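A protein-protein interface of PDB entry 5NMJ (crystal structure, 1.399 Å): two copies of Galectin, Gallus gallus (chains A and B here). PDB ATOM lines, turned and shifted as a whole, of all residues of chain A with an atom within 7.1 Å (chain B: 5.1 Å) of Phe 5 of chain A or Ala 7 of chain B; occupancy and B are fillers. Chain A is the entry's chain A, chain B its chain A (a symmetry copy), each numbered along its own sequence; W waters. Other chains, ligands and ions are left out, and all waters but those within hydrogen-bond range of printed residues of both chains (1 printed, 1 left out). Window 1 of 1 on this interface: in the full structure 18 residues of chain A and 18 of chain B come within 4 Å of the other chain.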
ATOM      1  N   ALA A   2     -34.478  21.979  30.501  1.00  0.00           N
ATOM      2  CA  ALA A   2     -34.654  22.463  29.137  1.00  0.00           C
ATOM      3  C   ALA A   2     -33.455  22.139  28.257  1.00  0.00           C
ATOM      4  O   ALA A   2     -32.306  22.404  28.611  1.00  0.00           O
ATOM      5  CB  ALA A   2     -34.919  23.956  29.132  1.00  0.00           C
ATOM      6  N   LEU A   3     -33.737  21.569  27.089  1.00  0.00           N
ATOM      7  CA  LEU A   3     -32.697  21.220  26.133  1.00  0.00           C
ATOM      8  C   LEU A   3     -32.148  22.474  25.458  1.00  0.00           C
ATOM      9  O   LEU A   3     -32.906  23.260  24.879  1.00  0.00           O
ATOM     10  CB  LEU A   3     -33.293  20.301  25.068  1.00  0.00           C
ATOM     11  CG  LEU A   3     -32.352  19.869  23.939  1.00  0.00           C
ATOM     12  CD1 LEU A   3     -31.267  18.976  24.491  1.00  0.00           C
ATOM     13  CD2 LEU A   3     -33.124  19.164  22.823  1.00  0.00           C
ATOM     14  N   ARG A   4     -30.832  22.655  25.512  1.00  0.00           N
ATOM     15  CA  ARG A   4     -30.201  23.787  24.845  1.00  0.00           C
ATOM     16  C   ARG A   4     -29.513  23.405  23.544  1.00  0.00           C
ATOM     17  O   ARG A   4     -29.429  24.242  22.638  1.00  0.00           O
ATOM     18  CB  ARG A   4     -29.201  24.492  25.776  1.00  0.00           C
ATOM     19  CG  ARG A   4     -29.714  24.779  27.191  1.00  0.00           C
ATOM     20  CD  ARG A   4     -30.957  25.679  27.204  1.00  0.00           C
ATOM     21  NE  ARG A   4     -30.691  27.069  26.828  1.00  0.00           N
ATOM     22  CZ  ARG A   4     -30.431  28.046  27.694  1.00  0.00           C
ATOM     23  NH1 ARG A   4     -30.395  27.793  28.992  1.00  0.00           N
ATOM     24  NH2 ARG A   4     -30.214  29.283  27.265  1.00  0.00           N
ATOM     25  N   PHE A   5     -29.040  22.167  23.425  1.00  0.00           N
ATOM     26  CA  PHE A   5     -28.359  21.734  22.215  1.00  0.00           C
ATOM     27  C   PHE A   5     -28.347  20.213  22.189  1.00  0.00           C
ATOM     28  O   PHE A   5     -28.174  19.572  23.226  1.00  0.00           O
ATOM     29  CB  PHE A   5     -26.921  22.277  22.186  1.00  0.00           C
ATOM     30  CG  PHE A   5     -26.135  21.856  20.977  1.00  0.00           C
ATOM     31  CD1 PHE A   5     -26.120  22.633  19.835  1.00  0.00           C
ATOM     32  CD2 PHE A   5     -25.404  20.677  20.993  1.00  0.00           C
ATOM     33  CE1 PHE A   5     -25.393  22.240  18.713  1.00  0.00           C
ATOM     34  CE2 PHE A   5     -24.669  20.281  19.878  1.00  0.00           C
ATOM     35  CZ  PHE A   5     -24.665  21.071  18.741  1.00  0.00           C
ATOM     36  N   GLU A   6     -28.537  19.643  21.009  1.00  0.00           N
ATOM     37  CA  GLU A   6     -28.377  18.204  20.832  1.00  0.00           C
ATOM     38  C   GLU A   6     -27.668  17.949  19.512  1.00  0.00           C
ATOM     39  O   GLU A   6     -27.906  18.654  18.527  1.00  0.00           O
ATOM     40  CB  GLU A   6     -29.741  17.503  20.849  1.00  0.00           C
ATOM     41  CG  GLU A   6     -29.706  16.002  20.559  1.00  0.00           C
ATOM     42  CD  GLU A   6     -31.088  15.374  20.652  1.00  0.00           C
ATOM     43  OE1 GLU A   6     -31.794  15.628  21.651  1.00  0.00           O
ATOM     44  OE2 GLU A   6     -31.475  14.638  19.720  1.00  0.00           O
ATOM     45  N   ALA A   7     -26.810  16.936  19.483  1.00  0.00           N
ATOM     46  CA  ALA A   7     -26.171  16.529  18.240  1.00  0.00           C
ATOM     47  C   ALA A   7     -26.197  15.014  18.145  1.00  0.00           C
ATOM     48  O   ALA A   7     -26.127  14.309  19.155  1.00  0.00           O
ATOM     49  CB  ALA A   7     -24.722  17.029  18.164  1.00  0.00           C
ATOM     50  N   LEU A   8     -26.314  14.522  16.914  1.00  0.00           N
ATOM     51  CA  LEU A   8     -26.381  13.092  16.623  1.00  0.00           C
ATOM     52  C   LEU A   8     -25.383  12.771  15.522  1.00  0.00           C
ATOM     53  O   LEU A   8     -25.397  13.411  14.465  1.00  0.00           O
ATOM     54  CB  LEU A   8     -27.797  12.715  16.160  1.00  0.00           C
ATOM     55  CG  LEU A   8     -27.996  11.293  15.626  1.00  0.00           C
ATOM     56  CD1 LEU A   8     -27.834  10.262  16.739  1.00  0.00           C
ATOM     57  CD2 LEU A   8     -29.361  11.160  14.953  1.00  0.00           C
ATOM     58  N   VAL A  19     -15.404  17.009  22.158  1.00  0.00           N
ATOM     59  CA  VAL A  19     -16.520  17.945  22.162  1.00  0.00           C
ATOM     60  C   VAL A  19     -16.063  19.170  22.942  1.00  0.00           C
ATOM     61  O   VAL A  19     -15.625  19.051  24.095  1.00  0.00           O
ATOM     62  CB  VAL A  19     -17.777  17.329  22.794  1.00  0.00           C
ATOM     63  CG1 VAL A  19     -18.899  18.366  22.890  1.00  0.00           C
ATOM     64  CG2 VAL A  19     -18.225  16.098  21.997  1.00  0.00           C
ATOM     65  N   VAL A  21     -17.342  22.856  24.236  1.00  0.00           N
ATOM     66  CA  VAL A  21     -18.526  23.671  24.479  1.00  0.00           C
ATOM     67  C   VAL A  21     -18.053  24.972  25.102  1.00  0.00           C
ATOM     68  O   VAL A  21     -17.359  24.958  26.129  1.00  0.00           O
ATOM     69  CB  VAL A  21     -19.512  22.965  25.419  1.00  0.00           C
ATOM     70  CG1 VAL A  21     -20.705  23.869  25.702  1.00  0.00           C
ATOM     71  CG2 VAL A  21     -19.957  21.644  24.839  1.00  0.00           C
ATOM     72  N   GLU A  33     -25.883  20.517  32.356  1.00  0.00           N
ATOM     73  CA  GLU A  33     -25.283  19.215  32.146  1.00  0.00           C
ATOM     74  C   GLU A  33     -24.951  18.998  30.683  1.00  0.00           C
ATOM     75  O   GLU A  33     -25.608  19.528  29.785  1.00  0.00           O
ATOM     76  CB  GLU A  33     -26.126  18.066  32.715  1.00  0.00           C
ATOM     77  CG  GLU A  33     -27.533  17.993  32.203  1.00  0.00           C
ATOM     78  CD  GLU A  33     -28.421  17.113  33.074  1.00  0.00           C
ATOM     79  OE1 GLU A  33     -28.673  15.958  32.684  1.00  0.00           O
ATOM     80  OE2 GLU A  33     -28.870  17.568  34.151  1.00  0.00           O
ATOM     81  N   LEU A 120     -25.193  13.671  21.824  1.00  0.00           N
ATOM     82  CA  LEU A 120     -24.756  14.620  22.833  1.00  0.00           C
ATOM     83  C   LEU A 120     -25.949  15.508  23.150  1.00  0.00           C
ATOM     84  O   LEU A 120     -26.626  15.975  22.235  1.00  0.00           O
ATOM     85  CB  LEU A 120     -23.650  15.498  22.241  1.00  0.00           C
ATOM     86  CG  LEU A 120     -23.299  16.786  22.991  1.00  0.00           C
ATOM     87  CD1 LEU A 120     -22.431  16.459  24.194  1.00  0.00           C
ATOM     88  CD2 LEU A 120     -22.609  17.791  22.077  1.00  0.00           C
ATOM     89  N   GLN A 121     -26.236  15.725  24.428  1.00  0.00           N
ATOM     90  CA  GLN A 121     -27.277  16.666  24.822  1.00  0.00           C
ATOM     91  C   GLN A 121     -26.716  17.625  25.859  1.00  0.00           C
ATOM     92  O   GLN A 121     -25.970  17.216  26.751  1.00  0.00           O
ATOM     93  CB  GLN A 121     -28.535  15.961  25.375  1.00  0.00           C
ATOM     94  CG  GLN A 121     -29.373  15.253  24.308  1.00  0.00           C
ATOM     95  CD  GLN A 121     -30.720  14.766  24.813  1.00  0.00           C
ATOM     96  OE1 GLN A 121     -30.897  14.504  26.002  1.00  0.00           O
ATOM     97  NE2 GLN A 121     -31.681  14.647  23.905  1.00  0.00           N
ATOM     98  N   ILE A 122     -27.074  18.898  25.737  1.00  0.00           N
ATOM     99  CA  ILE A 122     -26.660  19.920  26.686  1.00  0.00           C
ATOM    100  C   ILE A 122     -27.933  20.540  27.245  1.00  0.00           C
ATOM    101  O   ILE A 122     -28.795  20.981  26.477  1.00  0.00           O
ATOM    102  CB  ILE A 122     -25.766  20.982  26.023  1.00  0.00           C
ATOM    103  CG1 ILE A 122     -24.548  20.328  25.344  1.00  0.00           C
ATOM    104  CG2 ILE A 122     -25.346  22.036  27.050  1.00  0.00           C
ATOM    105  CD1 ILE A 122     -23.683  21.291  24.539  1.00  0.00           C
ATOM    106  N   LEU A 123     -28.064  20.547  28.567  1.00  0.00           N
ATOM    107  CA  LEU A 123     -29.321  20.911  29.208  1.00  0.00           C
ATOM    108  C   LEU A 123     -29.118  21.990  30.262  1.00  0.00           C
ATOM    109  O   LEU A 123     -28.055  22.089  30.885  1.00  0.00           O
ATOM    110  CB  LEU A 123     -29.975  19.705  29.909  1.00  0.00           C
ATOM    111  CG  LEU A 123     -30.088  18.386  29.146  1.00  0.00           C
ATOM    112  CD1 LEU A 123     -30.602  17.287  30.075  1.00  0.00           C
ATOM    113  CD2 LEU A 123     -30.982  18.514  27.941  1.00  0.00           C
ATOM    114  N   ILE A 126     -27.053  27.024  30.694  1.00  0.00           N
ATOM    115  CA  ILE A 126     -25.866  27.398  29.937  1.00  0.00           C
ATOM    116  C   ILE A 126     -26.320  28.143  28.693  1.00  0.00           C
ATOM    117  O   ILE A 126     -27.208  27.675  27.970  1.00  0.00           O
ATOM    118  CB  ILE A 126     -24.990  26.185  29.577  1.00  0.00           C
ATOM    119  CG1 ILE A 126     -23.809  26.634  28.718  1.00  0.00           C
ATOM    120  CG2 ILE A 126     -25.809  25.104  28.877  1.00  0.00           C
ATOM    121  CD1 ILE A 126     -22.815  25.519  28.405  1.00  0.00           C
ATOM    122  N   ILE A 128     -25.062  28.981  25.329  1.00  0.00           N
ATOM    123  CA  ILE A 128     -24.013  28.430  24.477  1.00  0.00           C
ATOM    124  C   ILE A 128     -23.561  29.471  23.461  1.00  0.00           C
ATOM    125  O   ILE A 128     -24.384  30.128  22.811  1.00  0.00           O
ATOM    126  CB  ILE A 128     -24.522  27.164  23.771  1.00  0.00           C
ATOM    127  CG1 ILE A 128     -24.844  26.077  24.799  1.00  0.00           C
ATOM    128  CG2 ILE A 128     -23.495  26.665  22.758  1.00  0.00           C
ATOM    129  CD1 ILE A 128     -25.636  24.888  24.231  1.00  0.00           C
ATOM    130  N   SER A 130     -20.681  28.272  21.409  1.00  0.00           N
ATOM    131  CA  SER A 130     -20.080  27.421  20.386  1.00  0.00           C
ATOM    132  C   SER A 130     -20.132  25.970  20.847  1.00  0.00           C
ATOM    133  O   SER A 130     -19.938  25.691  22.037  1.00  0.00           O
ATOM    134  CB  SER A 130     -18.612  27.801  20.152  1.00  0.00           C
ATOM    135  OG  SER A 130     -18.033  27.004  19.132  1.00  0.00           O
ATOM    136  N   VAL A 131     -20.365  25.054  19.905  1.00  0.00           N
ATOM    137  CA  VAL A 131     -20.175  23.622  20.119  1.00  0.00           C
ATOM    138  C   VAL A 131     -19.373  23.105  18.935  1.00  0.00           C
ATOM    139  O   VAL A 131     -19.776  23.296  17.779  1.00  0.00           O
ATOM    140  CB  VAL A 131     -21.484  22.829  20.257  1.00  0.00           C
ATOM    141  CG1 VAL A 131     -21.151  21.347  20.507  1.00  0.00           C
ATOM    142  CG2 VAL A 131     -22.346  23.366  21.397  1.00  0.00           C
ATOM    143  N   GLU A 132     -18.235  22.477  19.216  1.00  0.00           N
ATOM    144  CA  GLU A 132     -17.396  21.870  18.192  1.00  0.00           C
ATOM    145  C   GLU A 132     -17.289  20.390  18.506  1.00  0.00           C
ATOM    146  O   GLU A 132     -17.008  20.016  19.649  1.00  0.00           O
ATOM    147  CB  GLU A 132     -16.002  22.499  18.191  1.00  0.00           C
ATOM    148  CG  GLU A 132     -15.005  21.831  17.240  1.00  0.00           C
ATOM    149  CD  GLU A 132     -13.557  22.219  17.510  1.00  0.00           C
ATOM    150  OE1 GLU A 132     -13.312  23.199  18.247  1.00  0.00           O
ATOM    151  OE2 GLU A 132     -12.655  21.533  16.986  1.00  0.00           O
ATOM    152  N   ILE A 133     -17.519  19.551  17.503  1.00  0.00           N
ATOM    153  CA  ILE A 133     -17.426  18.101  17.655  1.00  0.00           C
ATOM    154  C   ILE A 133     -16.415  17.642  16.615  1.00  0.00           C
ATOM    155  O   ILE A 133     -16.657  17.769  15.404  1.00  0.00           O
ATOM    156  CB  ILE A 133     -18.790  17.420  17.477  1.00  0.00           C
ATOM    157  CG1 ILE A 133     -19.774  17.958  18.531  1.00  0.00           C
ATOM    158  CG2 ILE A 133     -18.642  15.903  17.572  1.00  0.00           C
ATOM    159  CD1 ILE A 133     -21.224  17.618  18.280  1.00  0.00           C
ATOM    160  N   PHE B   5     -25.000  13.493  10.211  1.00  0.00           N
ATOM    161  CA  PHE B   5     -24.898  14.343  11.386  1.00  0.00           C
ATOM    162  C   PHE B   5     -26.150  15.203  11.468  1.00  0.00           C
ATOM    163  O   PHE B   5     -26.657  15.666  10.445  1.00  0.00           O
ATOM    164  CB  PHE B   5     -23.648  15.234  11.296  1.00  0.00           C
ATOM    165  CG  PHE B   5     -23.478  16.165  12.463  1.00  0.00           C
ATOM    166  CD1 PHE B   5     -22.747  15.786  13.572  1.00  0.00           C
ATOM    167  CD2 PHE B   5     -24.050  17.428  12.440  1.00  0.00           C
ATOM    168  CE1 PHE B   5     -22.591  16.649  14.655  1.00  0.00           C
ATOM    169  CE2 PHE B   5     -23.895  18.299  13.516  1.00  0.00           C
ATOM    170  CZ  PHE B   5     -23.159  17.904  14.620  1.00  0.00           C
ATOM    171  N   GLU B   6     -26.648  15.407  12.678  1.00  0.00           N
ATOM    172  CA  GLU B   6     -27.739  16.349  12.896  1.00  0.00           C
ATOM    173  C   GLU B   6     -27.467  17.127  14.172  1.00  0.00           C
ATOM    174  O   GLU B   6     -26.946  16.572  15.145  1.00  0.00           O
ATOM    175  CB  GLU B   6     -29.079  15.608  12.999  1.00  0.00           C
ATOM    176  CG  GLU B   6     -30.283  16.485  13.341  1.00  0.00           C
ATOM    177  CD  GLU B   6     -31.577  15.686  13.366  1.00  0.00           C
ATOM    178  OE1 GLU B   6     -31.827  14.922  12.410  1.00  0.00           O
ATOM    179  OE2 GLU B   6     -32.338  15.810  14.349  1.00  0.00           O
ATOM    180  N   ALA B   7     -27.829  18.405  14.180  1.00  0.00           N
ATOM    181  CA  ALA B   7     -27.725  19.207  15.390  1.00  0.00           C
ATOM    182  C   ALA B   7     -28.990  20.035  15.542  1.00  0.00           C
ATOM    183  O   ALA B   7     -29.605  20.449  14.556  1.00  0.00           O
ATOM    184  CB  ALA B   7     -26.502  20.133  15.347  1.00  0.00           C
ATOM    185  N   LEU B   8     -29.378  20.257  16.795  1.00  0.00           N
ATOM    186  CA  LEU B   8     -30.581  21.010  17.143  1.00  0.00           C
ATOM    187  C   LEU B   8     -30.217  22.057  18.184  1.00  0.00           C
ATOM    188  O   LEU B   8     -29.621  21.727  19.215  1.00  0.00           O
ATOM    189  CB  LEU B   8     -31.647  20.063  17.715  1.00  0.00           C
ATOM    190  CG  LEU B   8     -32.899  20.710  18.314  1.00  0.00           C
ATOM    191  CD1 LEU B   8     -33.741  21.380  17.231  1.00  0.00           C
ATOM    192  CD2 LEU B   8     -33.720  19.678  19.084  1.00  0.00           C
ATOM    193  N   TYR B   9     -30.579  23.315  17.921  1.00  0.00           N
ATOM    194  CA  TYR B   9     -30.351  24.423  18.848  1.00  0.00           C
ATOM    195  C   TYR B   9     -31.693  25.135  18.944  1.00  0.00           C
ATOM    196  O   TYR B   9     -32.008  25.996  18.114  1.00  0.00           O
ATOM    197  CB  TYR B   9     -29.241  25.350  18.343  1.00  0.00           C
ATOM    198  CG  TYR B   9     -28.989  26.529  19.248  1.00  0.00           C
ATOM    199  CD1 TYR B   9     -28.333  26.375  20.462  1.00  0.00           C
ATOM    200  CD2 TYR B   9     -29.433  27.802  18.901  1.00  0.00           C
ATOM    201  CE1 TYR B   9     -28.124  27.441  21.293  1.00  0.00           C
ATOM    202  CE2 TYR B   9     -29.234  28.879  19.736  1.00  0.00           C
ATOM    203  CZ  TYR B   9     -28.572  28.695  20.932  1.00  0.00           C
ATOM    204  OH  TYR B   9     -28.366  29.772  21.776  1.00  0.00           O
ATOM    205  N   PRO B  10     -32.530  24.767  19.917  1.00  0.00           N
ATOM    206  CA  PRO B  10     -33.939  25.207  19.885  1.00  0.00           C
ATOM    207  C   PRO B  10     -34.152  26.705  19.955  1.00  0.00           C
ATOM    208  O   PRO B  10     -35.234  27.162  19.567  1.00  0.00           O
ATOM    209  CB  PRO B  10     -34.559  24.493  21.094  1.00  0.00           C
ATOM    210  CG  PRO B  10     -33.747  23.228  21.202  1.00  0.00           C
ATOM    211  CD  PRO B  10     -32.333  23.672  20.886  1.00  0.00           C
ATOM    212  N   MET B  13     -30.560  29.155  15.481  1.00  0.00           N
ATOM    213  CA  MET B  13     -29.161  29.338  15.097  1.00  0.00           C
ATOM    214  C   MET B  13     -29.020  30.200  13.840  1.00  0.00           C
ATOM    215  O   MET B  13     -28.187  29.932  12.973  1.00  0.00           O
ATOM    216  CB  MET B  13     -28.420  28.002  14.978  1.00  0.00           C
ATOM    217  CG  MET B  13     -29.039  27.002  13.998  1.00  0.00           C
ATOM    218  SD  MET B  13     -27.976  25.565  13.634  1.00  0.00           S
ATOM    219  CE  MET B  13     -28.617  24.340  14.763  1.00  0.00           C
ATOM    220  N   THR B 118     -33.614  26.029  13.471  1.00  0.00           N
ATOM    221  CA  THR B 118     -33.080  25.418  14.681  1.00  0.00           C
ATOM    222  C   THR B 118     -32.288  24.151  14.419  1.00  0.00           C
ATOM    223  O   THR B 118     -31.681  23.628  15.357  1.00  0.00           O
ATOM    224  CB  THR B 118     -34.226  25.044  15.634  1.00  0.00           C
ATOM    225  OG1 THR B 118     -35.102  24.132  14.954  1.00  0.00           O
ATOM    226  CG2 THR B 118     -35.007  26.282  16.069  1.00  0.00           C
ATOM    227  N   LYS B 119     -32.302  23.617  13.202  1.00  0.00           N
ATOM    228  CA  LYS B 119     -31.773  22.280  12.982  1.00  0.00           C
ATOM    229  C   LYS B 119     -30.879  22.256  11.756  1.00  0.00           C
ATOM    230  O   LYS B 119     -31.160  22.916  10.752  1.00  0.00           O
ATOM    231  CB  LYS B 119     -32.907  21.249  12.864  1.00  0.00           C
ATOM    232  CG  LYS B 119     -32.416  19.821  12.718  1.00  0.00           C
ATOM    233  CD  LYS B 119     -33.402  18.824  13.301  1.00  0.00           C
ATOM    234  CE  LYS B 119     -34.634  18.674  12.433  1.00  0.00           C
ATOM    235  NZ  LYS B 119     -35.556  17.638  12.985  1.00  0.00           N
ATOM    236  N   LEU B 120     -29.800  21.480  11.854  1.00  0.00           N
ATOM    237  CA  LEU B 120     -28.840  21.276  10.783  1.00  0.00           C
ATOM    238  C   LEU B 120     -28.788  19.781  10.517  1.00  0.00           C
ATOM    239  O   LEU B 120     -28.712  18.992  11.459  1.00  0.00           O
ATOM    240  CB  LEU B 120     -27.458  21.726  11.265  1.00  0.00           C
ATOM    241  CG  LEU B 120     -26.247  21.271  10.446  1.00  0.00           C
ATOM    242  CD1 LEU B 120     -26.119  22.129   9.198  1.00  0.00           C
ATOM    243  CD2 LEU B 120     -24.967  21.316  11.273  1.00  0.00           C
ATOM    244  N   ILE B 133     -20.370  24.722  15.417  1.00  0.00           N
ATOM    245  CA  ILE B 133     -21.530  25.602  15.313  1.00  0.00           C
ATOM    246  C   ILE B 133     -21.278  26.735  16.297  1.00  0.00           C
ATOM    247  O   ILE B 133     -21.224  26.509  17.516  1.00  0.00           O
ATOM    248  CB  ILE B 133     -22.839  24.858  15.610  1.00  0.00           C
ATOM    249  CG1 ILE B 133     -23.013  23.704  14.607  1.00  0.00           C
ATOM    250  CG2 ILE B 133     -24.022  25.823  15.560  1.00  0.00           C
ATOM    251  CD1 ILE B 133     -24.081  22.700  14.969  1.00  0.00           C
HETATM  252  O   HOH W   1     -26.657  31.272  23.468  1.00  0.00           O
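The backbone NH (N) of Leu 8 of chain A sits at hydrogen-bond distance from the backbone carbonyl oxygen (O) of Glu 6 of chain B (2.8 Å). The backbone carbonyl oxygen (O) of Val 131 of chain A sits at hydrogen-bond distance from the backbone NH (N) of Ile 133 of chain B, at 2.8 Å. O of Glu 6 of chain A sits at hydrogen-bond distance from N of Leu 8 of chain B (2.8 Å).
OE1 of Glu 6 of chain A is in hydrogen-bond range of NE2 of Gln 121 of chain A, at 2.5 Å. The backbone carbonyl oxygen of Ala 7 of chain B lies within hydrogen-bond range of the backbone NH of Leu 120 of chain B, 2.9 Å away. O of Ala 7 of chain A is in hydrogen-bond range of N of Leu 120 of chain A (2.9 Å). O of Ile 122 of chain A is in hydrogen-bond range of N of Arg 4 of chain A (2.8 Å). N of Ile 122 of chain A sits at hydrogen-bond distance from O of Phe 5 of chain A (2.8 Å). The backbone NH of Tyr 9 of chain B sits at hydrogen-bond distance from the backbone carbonyl oxygen of Thr 118 of chain B.
Leu 8 of chain B touches Leu 3 of chain A. CG of Pro 10 of chain B touches O of Leu 3 of chain A, 3.8 Å away. Tyr 9 of chain B touches Arg 4 of chain A (CD1 to O, 3.2 Å). Ala 7 of chain B touches Phe 5 of chain A. Phe 5 of chain A touches Leu 8 of chain B. Phe 5 of chain A touches Ile 133 of chain B (CE1 to CD1, 3.99 Å). Ala 7 of chain A touches Phe 5 of chain B (CB to CZ, 3.97 Å). Leu 8 of chain A touches Phe 5 of chain B (O to CA, 3.3 Å). CA of Ser 130 of chain A touches O of Ile 133 of chain B, at 3.2 Å. CD1 of Ile 133 of chain A touches CE1 of Phe 5 of chain B, at 3.99 Å.
Printed residues of chain B within 4 Å of Arg 4 of chain A: Tyr 9 (3.2 Å) and Pro 10 (3.4 Å). Printed residues of chain B within 4 Å of Phe 5 of chain A: Ala 7 (3.97 Å), Leu 8 (3.3 Å) and Ile 133 (3.99 Å). Of the printed residues of chain A, Phe 5 of chain B touches Ala 7, Leu 8 and Ile 133. Of chain A, only Phe 5 (3.97 Å) and Glu 6 (3.2 Å) come within 4 Å of Ala 7 of chain B. Met 13 of chain B touches none of the printed residues of chain A. Thr 118 of chain B touches none of the printed residues of chain A. The nearest printed residue of chain B that does not touch Phe 5 of chain A is Tyr 9 of chain B (4.4 Å). The nearest residue of chain A that does not touch Ala 7 of chain B is Ala 7 of chain A (4.2 Å).
Of the 11 printed residues of chain B, 7 touch a printed residue of chain A. Hydrophobic or aromatic side chains of chain B that line the printed part of chain A: Phe 5, Ala 7, Leu 8, Tyr 9, Pro 10 and Ile 133. Hydrophobic or aromatic side chains of chain A within 4 Å of the printed part of chain B: Leu 3, Phe 5, Ala 7 and Ile 133. Among the printed residues, no Asp or Glu carboxylate lies within 4 Å of a Lys or Arg side-chain nitrogen of the other chain.
Phe 5 of chain A touches Ala 7 of chain B, and with the chains exchanged Ala 7 of chain A touches Phe 5 of chain B. Phe 5 of chain A touches Leu 8 of chain B, and with the chains exchanged Leu 8 of chain A touches Phe 5 of chain B. Phe 5 of chain A touches Ile 133 of chain B, and with the chains exchanged Ile 133 of chain A touches Phe 5 of chain B. Glu 6 of chain A touches Ala 7 of chain B, and with the chains exchanged Ala 7 of chain A touches Glu 6 of chain B. 6 positions are printed for both chains. Of the 16 pairs that touch across the chains among the printed residues, 10 have their exchanged pair printed and touching as well.
Water W1 lies within hydrogen-bond range of O of Ile 128 of chain A (2.6 Å) and OH of Tyr 9 of chain B (2.8 Å).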
